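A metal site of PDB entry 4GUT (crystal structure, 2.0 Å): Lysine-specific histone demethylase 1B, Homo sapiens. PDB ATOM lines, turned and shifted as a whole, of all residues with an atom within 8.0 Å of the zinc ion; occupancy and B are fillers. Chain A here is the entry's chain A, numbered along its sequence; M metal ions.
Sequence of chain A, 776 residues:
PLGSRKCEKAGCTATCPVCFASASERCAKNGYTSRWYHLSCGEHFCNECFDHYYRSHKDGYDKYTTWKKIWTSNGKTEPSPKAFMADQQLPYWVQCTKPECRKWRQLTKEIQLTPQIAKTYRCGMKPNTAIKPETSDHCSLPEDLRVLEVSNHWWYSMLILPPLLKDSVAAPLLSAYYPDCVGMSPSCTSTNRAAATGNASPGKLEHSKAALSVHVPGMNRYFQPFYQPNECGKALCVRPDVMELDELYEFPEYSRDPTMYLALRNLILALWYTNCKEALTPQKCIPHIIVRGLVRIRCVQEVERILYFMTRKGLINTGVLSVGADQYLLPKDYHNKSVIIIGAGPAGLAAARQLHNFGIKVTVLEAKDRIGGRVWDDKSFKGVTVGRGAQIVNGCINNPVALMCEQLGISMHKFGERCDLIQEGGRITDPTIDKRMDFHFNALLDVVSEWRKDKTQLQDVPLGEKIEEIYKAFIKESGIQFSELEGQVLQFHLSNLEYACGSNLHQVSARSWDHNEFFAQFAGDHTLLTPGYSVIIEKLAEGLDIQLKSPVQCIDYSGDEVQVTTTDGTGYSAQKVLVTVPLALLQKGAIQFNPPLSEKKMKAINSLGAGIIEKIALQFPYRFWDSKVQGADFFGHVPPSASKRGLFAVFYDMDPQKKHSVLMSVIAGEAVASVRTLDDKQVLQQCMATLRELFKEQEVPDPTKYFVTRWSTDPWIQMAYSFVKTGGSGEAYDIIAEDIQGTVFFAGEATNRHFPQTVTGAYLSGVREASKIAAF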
ATOM      1  N   GLN A  95       8.200  22.165  14.375  1.00  0.00           N
ATOM      2  CA  GLN A  95       7.321  23.311  14.134  1.00  0.00           C
ATOM      3  C   GLN A  95       8.049  24.366  13.313  1.00  0.00           C
ATOM      4  O   GLN A  95       9.196  24.698  13.583  1.00  0.00           O
ATOM      5  CB  GLN A  95       6.836  23.895  15.462  1.00  0.00           C
ATOM      6  CG  GLN A  95       5.546  24.700  15.361  1.00  0.00           C
ATOM      7  CD  GLN A  95       4.988  25.122  16.715  1.00  0.00           C
ATOM      8  OE1 GLN A  95       5.512  24.763  17.766  1.00  0.00           O
ATOM      9  NE2 GLN A  95       3.893  25.873  16.681  1.00  0.00           N
ATOM     10  N   CYS A  96       7.362  24.880  12.292  1.00  0.00           N
ATOM     11  CA  CYS A  96       7.880  25.976  11.493  1.00  0.00           C
ATOM     12  C   CYS A  96       8.077  27.190  12.389  1.00  0.00           C
ATOM     13  O   CYS A  96       7.193  27.524  13.178  1.00  0.00           O
ATOM     14  CB  CYS A  96       6.912  26.320  10.368  1.00  0.00           C
ATOM     15  SG  CYS A  96       7.476  27.684   9.331  1.00  0.00           S
ATOM     16  N   THR A  97       9.213  27.850  12.250  1.00  0.00           N
ATOM     17  CA  THR A  97       9.564  28.976  13.116  1.00  0.00           C
ATOM     18  C   THR A  97       9.150  30.328  12.537  1.00  0.00           C
ATOM     19  O   THR A  97       9.389  31.368  13.154  1.00  0.00           O
ATOM     20  CB  THR A  97      11.061  28.990  13.465  1.00  0.00           C
ATOM     21  OG1 THR A  97      11.834  29.099  12.267  1.00  0.00           O
ATOM     22  CG2 THR A  97      11.444  27.725  14.211  1.00  0.00           C
ATOM     23  N   LYS A  98       8.531  30.318  11.362  1.00  0.00           N
ATOM     24  CA  LYS A  98       7.946  31.528  10.799  1.00  0.00           C
ATOM     25  C   LYS A  98       6.759  31.931  11.672  1.00  0.00           C
ATOM     26  O   LYS A  98       5.807  31.168  11.804  1.00  0.00           O
ATOM     27  CB  LYS A  98       7.491  31.308   9.356  1.00  0.00           C
ATOM     28  CG  LYS A  98       7.102  32.589   8.636  1.00  0.00           C
ATOM     29  CD  LYS A  98       6.469  32.316   7.277  1.00  0.00           C
ATOM     30  CE  LYS A  98       6.330  33.621   6.498  1.00  0.00           C
ATOM     31  NZ  LYS A  98       5.375  33.517   5.371  1.00  0.00           N
ATOM     32  N   PRO A  99       6.830  33.125  12.297  1.00  0.00           N
ATOM     33  CA  PRO A  99       5.865  33.586  13.302  1.00  0.00           C
ATOM     34  C   PRO A  99       4.403  33.562  12.851  1.00  0.00           C
ATOM     35  O   PRO A  99       3.508  33.356  13.677  1.00  0.00           O
ATOM     36  CB  PRO A  99       6.292  35.035  13.563  1.00  0.00           C
ATOM     37  CG  PRO A  99       7.733  35.077  13.185  1.00  0.00           C
ATOM     38  CD  PRO A  99       7.856  34.144  12.009  1.00  0.00           C
ATOM     39  N   GLU A 100       4.168  33.766  11.557  1.00  0.00           N
ATOM     40  CA  GLU A 100       2.808  33.787  11.009  1.00  0.00           C
ATOM     41  C   GLU A 100       2.343  32.415  10.473  1.00  0.00           C
ATOM     42  O   GLU A 100       1.158  32.225  10.199  1.00  0.00           O
ATOM     43  CB  GLU A 100       2.647  34.876   9.939  1.00  0.00           C
ATOM     44  CG  GLU A 100       3.786  34.992   8.941  1.00  0.00           C
ATOM     45  CD  GLU A 100       4.887  35.948   9.374  1.00  0.00           C
ATOM     46  OE1 GLU A 100       6.061  35.516   9.463  1.00  0.00           O
ATOM     47  OE2 GLU A 100       4.587  37.128   9.648  1.00  0.00           O
ATOM     48  N   CYS A 101       3.284  31.479  10.337  1.00  0.00           N
ATOM     49  CA  CYS A 101       2.958  30.110   9.942  1.00  0.00           C
ATOM     50  C   CYS A 101       2.768  29.248  11.190  1.00  0.00           C
ATOM     51  O   CYS A 101       1.645  28.907  11.543  1.00  0.00           O
ATOM     52  CB  CYS A 101       4.053  29.514   9.040  1.00  0.00           C
ATOM     53  SG  CYS A 101       3.846  27.769   8.599  1.00  0.00           S
ATOM     54  N   ARG A 102       3.876  28.914  11.851  1.00  0.00           N
ATOM     55  CA  ARG A 102       3.884  28.146  13.103  1.00  0.00           C
ATOM     56  C   ARG A 102       3.272  26.735  12.993  1.00  0.00           C
ATOM     57  O   ARG A 102       2.839  26.166  14.008  1.00  0.00           O
ATOM     58  CB  ARG A 102       3.249  28.948  14.252  1.00  0.00           C
ATOM     59  CG  ARG A 102       3.999  30.224  14.636  1.00  0.00           C
ATOM     60  CD  ARG A 102       5.423  29.952  15.096  1.00  0.00           C
ATOM     61  NE  ARG A 102       5.457  29.366  16.439  1.00  0.00           N
ATOM     62  CZ  ARG A 102       6.334  28.449  16.846  1.00  0.00           C
ATOM     63  NH1 ARG A 102       6.266  27.989  18.089  1.00  0.00           N
ATOM     64  NH2 ARG A 102       7.276  27.980  16.021  1.00  0.00           N
ATOM     65  N   LYS A 103       3.248  26.165  11.797  1.00  0.00           N
ATOM     66  CA  LYS A 103       2.638  24.844  11.638  1.00  0.00           C
ATOM     67  C   LYS A 103       3.604  23.703  11.923  1.00  0.00           C
ATOM     68  O   LYS A 103       4.797  23.815  11.681  1.00  0.00           O
ATOM     69  CB  LYS A 103       1.972  24.705  10.265  1.00  0.00           C
ATOM     70  CG  LYS A 103       0.673  25.499  10.137  1.00  0.00           C
ATOM     71  CD  LYS A 103      -0.200  25.023   8.981  1.00  0.00           C
ATOM     72  CE  LYS A 103       0.285  25.509   7.633  1.00  0.00           C
ATOM     73  NZ  LYS A 103      -0.145  26.899   7.321  1.00  0.00           N
ATOM     74  N   TRP A 104       3.072  22.617  12.463  1.00  0.00           N
ATOM     75  CA  TRP A 104       3.868  21.426  12.746  1.00  0.00           C
ATOM     76  C   TRP A 104       3.987  20.583  11.497  1.00  0.00           C
ATOM     77  O   TRP A 104       3.018  20.410  10.772  1.00  0.00           O
ATOM     78  CB  TRP A 104       3.222  20.616  13.854  1.00  0.00           C
ATOM     79  CG  TRP A 104       3.536  21.116  15.255  1.00  0.00           C
ATOM     80  CD1 TRP A 104       2.779  21.991  16.042  1.00  0.00           C
ATOM     81  CD2 TRP A 104       4.691  20.758  16.088  1.00  0.00           C
ATOM     82  NE1 TRP A 104       3.377  22.186  17.264  1.00  0.00           N
ATOM     83  CE2 TRP A 104       4.519  21.481  17.354  1.00  0.00           C
ATOM     84  CE3 TRP A 104       5.803  19.937  15.920  1.00  0.00           C
ATOM     85  CZ2 TRP A 104       5.439  21.372  18.395  1.00  0.00           C
ATOM     86  CZ3 TRP A 104       6.717  19.838  16.970  1.00  0.00           C
ATOM     87  CH2 TRP A 104       6.538  20.547  18.180  1.00  0.00           C
ATOM     88  N   ARG A 105       5.183  20.067  11.248  1.00  0.00           N
ATOM     89  CA  ARG A 105       5.454  19.276  10.044  1.00  0.00           C
ATOM     90  C   ARG A 105       6.167  17.976  10.403  1.00  0.00           C
ATOM     91  O   ARG A 105       7.039  17.963  11.285  1.00  0.00           O
ATOM     92  CB  ARG A 105       6.344  20.042   9.066  1.00  0.00           C
ATOM     93  CG  ARG A 105       5.933  21.469   8.760  1.00  0.00           C
ATOM     94  CD  ARG A 105       5.253  21.631   7.408  1.00  0.00           C
ATOM     95  NE  ARG A 105       3.801  21.502   7.486  1.00  0.00           N
ATOM     96  CZ  ARG A 105       2.935  22.204   6.748  1.00  0.00           C
ATOM     97  NH1 ARG A 105       3.350  23.119   5.891  1.00  0.00           N
ATOM     98  NH2 ARG A 105       1.634  22.008   6.906  1.00  0.00           N
ATOM     99  N   TYR A 121      13.967  25.628  11.783  1.00  0.00           N
ATOM    100  CA  TYR A 121      13.072  25.002  10.812  1.00  0.00           C
ATOM    101  C   TYR A 121      12.024  25.947  10.223  1.00  0.00           C
ATOM    102  O   TYR A 121      11.414  26.749  10.939  1.00  0.00           O
ATOM    103  CB  TYR A 121      12.368  23.770  11.382  1.00  0.00           C
ATOM    104  CG  TYR A 121      11.514  23.069  10.338  1.00  0.00           C
ATOM    105  CD1 TYR A 121      10.134  23.270  10.302  1.00  0.00           C
ATOM    106  CD2 TYR A 121      12.091  22.263   9.356  1.00  0.00           C
ATOM    107  CE1 TYR A 121       9.351  22.652   9.344  1.00  0.00           C
ATOM    108  CE2 TYR A 121      11.324  21.644   8.386  1.00  0.00           C
ATOM    109  CZ  TYR A 121       9.948  21.844   8.387  1.00  0.00           C
ATOM    110  OH  TYR A 121       9.168  21.235   7.432  1.00  0.00           O
ATOM    111  N   ARG A 122      11.846  25.868   8.914  1.00  0.00           N
ATOM    112  CA  ARG A 122      10.592  26.296   8.292  1.00  0.00           C
ATOM    113  C   ARG A 122      10.112  25.290   7.262  1.00  0.00           C
ATOM    114  O   ARG A 122      10.908  24.509   6.729  1.00  0.00           O
ATOM    115  CB  ARG A 122      10.623  27.726   7.723  1.00  0.00           C
ATOM    116  CG  ARG A 122      11.979  28.378   7.587  1.00  0.00           C
ATOM    117  CD  ARG A 122      11.925  29.785   8.162  1.00  0.00           C
ATOM    118  NE  ARG A 122      11.018  30.665   7.415  1.00  0.00           N
ATOM    119  CZ  ARG A 122      10.709  31.909   7.771  1.00  0.00           C
ATOM    120  NH1 ARG A 122      11.215  32.436   8.884  1.00  0.00           N
ATOM    121  NH2 ARG A 122       9.888  32.635   7.025  1.00  0.00           N
ATOM    122  N   CYS A 123       8.812  25.287   7.012  1.00  0.00           N
ATOM    123  CA  CYS A 123       8.180  24.387   6.060  1.00  0.00           C
ATOM    124  C   CYS A 123       9.009  24.295   4.794  1.00  0.00           C
ATOM    125  O   CYS A 123       9.446  25.311   4.250  1.00  0.00           O
ATOM    126  CB  CYS A 123       6.783  24.879   5.738  1.00  0.00           C
ATOM    127  SG  CYS A 123       5.731  25.040   7.188  1.00  0.00           S
ATOM    128  N   GLY A 124       9.234  23.065   4.331  1.00  0.00           N
ATOM    129  CA  GLY A 124       9.944  22.828   3.081  1.00  0.00           C
ATOM    130  C   GLY A 124      11.437  22.625   3.193  1.00  0.00           C
ATOM    131  O   GLY A 124      12.050  22.096   2.263  1.00  0.00           O
ATOM    132  N   ASP A 137       5.986  27.611  -1.996  1.00  0.00           N
ATOM    133  CA  ASP A 137       4.915  28.043  -1.076  1.00  0.00           C
ATOM    134  C   ASP A 137       4.583  27.020   0.016  1.00  0.00           C
ATOM    135  O   ASP A 137       3.417  26.797   0.344  1.00  0.00           O
ATOM    136  CB  ASP A 137       3.654  28.461  -1.834  1.00  0.00           C
ATOM    137  CG  ASP A 137       3.326  29.923  -1.636  1.00  0.00           C
ATOM    138  OD1 ASP A 137       3.523  30.434  -0.510  1.00  0.00           O
ATOM    139  OD2 ASP A 137       2.852  30.567  -2.602  1.00  0.00           O
ATOM    140  N   HIS A 138       5.630  26.437   0.593  1.00  0.00           N
ATOM    141  CA  HIS A 138       5.512  25.330   1.555  1.00  0.00           C
ATOM    142  C   HIS A 138       4.693  25.616   2.779  1.00  0.00           C
ATOM    143  O   HIS A 138       3.983  24.738   3.267  1.00  0.00           O
ATOM    144  CB  HIS A 138       6.904  24.837   1.951  1.00  0.00           C
ATOM    145  CG  HIS A 138       7.790  24.493   0.780  1.00  0.00           C
ATOM    146  ND1 HIS A 138       7.594  23.413   0.011  1.00  0.00           N
ATOM    147  CD2 HIS A 138       8.933  25.135   0.282  1.00  0.00           C
ATOM    148  CE1 HIS A 138       8.549  23.349  -0.939  1.00  0.00           C
ATOM    149  NE2 HIS A 138       9.367  24.401  -0.769  1.00  0.00           N
ATOM    150  N   CYS A 139       4.775  26.843   3.289  1.00  0.00           N
ATOM    151  CA  CYS A 139       4.017  27.251   4.490  1.00  0.00           C
ATOM    152  C   CYS A 139       2.502  27.280   4.260  1.00  0.00           C
ATOM    153  O   CYS A 139       1.732  27.097   5.209  1.00  0.00           O
ATOM    154  CB  CYS A 139       4.513  28.606   5.018  1.00  0.00           C
ATOM    155  SG  CYS A 139       6.127  28.564   5.853  1.00  0.00           S
ATOM    156  N   SER A 140       2.079  27.486   3.019  1.00  0.00           N
ATOM    157  CA  SER A 140       0.649  27.600   2.686  1.00  0.00           C
ATOM    158  C   SER A 140      -0.083  26.261   2.695  1.00  0.00           C
ATOM    159  O   SER A 140      -1.299  26.209   2.905  1.00  0.00           O
ATOM    160  CB  SER A 140       0.450  28.327   1.355  1.00  0.00           C
ATOM    161  OG  SER A 140       0.916  27.542   0.265  1.00  0.00           O
ATOM    162  N   LEU A 141       0.663  25.170   2.463  1.00  0.00           N
ATOM    163  CA  LEU A 141       0.095  23.819   2.503  1.00  0.00           C
ATOM    164  C   LEU A 141      -0.496  23.525   3.886  1.00  0.00           C
ATOM    165  O   LEU A 141       0.087  23.913   4.891  1.00  0.00           O
ATOM    166  CB  LEU A 141       1.160  22.774   2.155  1.00  0.00           C
ATOM    167  CG  LEU A 141       1.982  22.972   0.871  1.00  0.00           C
ATOM    168  CD1 LEU A 141       3.064  21.893   0.754  1.00  0.00           C
ATOM    169  CD2 LEU A 141       1.122  23.001  -0.383  1.00  0.00           C
HETATM  170 ZN    ZN M   1       5.666  27.404   7.733  1.00  0.00          ZN
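The guanidinium group (NH1) of Arg 105 sits close to the side-chain sulfur (SG) of Cys 123 (3.3 Å).
SG of Cys 96 lies close to N of Lys 98, 3.5 Å away.
SG of Cys 101 lies close to N of Lys 103 (3.6 Å).
The backbone carbonyl oxygen (O) of Cys 139 sits at hydrogen-bond distance from the side-chain amino group (NZ) of Lys 103 (2.8 Å).
The backbone carbonyl oxygen of Cys 96 is in hydrogen-bond range of the guanidinium group of Arg 102 (2.9 Å).
The backbone carbonyl oxygen (O) of Lys 103 is in hydrogen-bond range of the backbone NH (N) of Cys 96 (2.8 Å).
The zinc ion is bound by the side-chain sulfur of Cys 101 (2.0 Å), the side-chain sulfur of Cys 139 (2.3 Å), the side-chain sulfur of Cys 123 (2.4 Å) and the side-chain sulfur of Cys 96 (2.4 Å).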
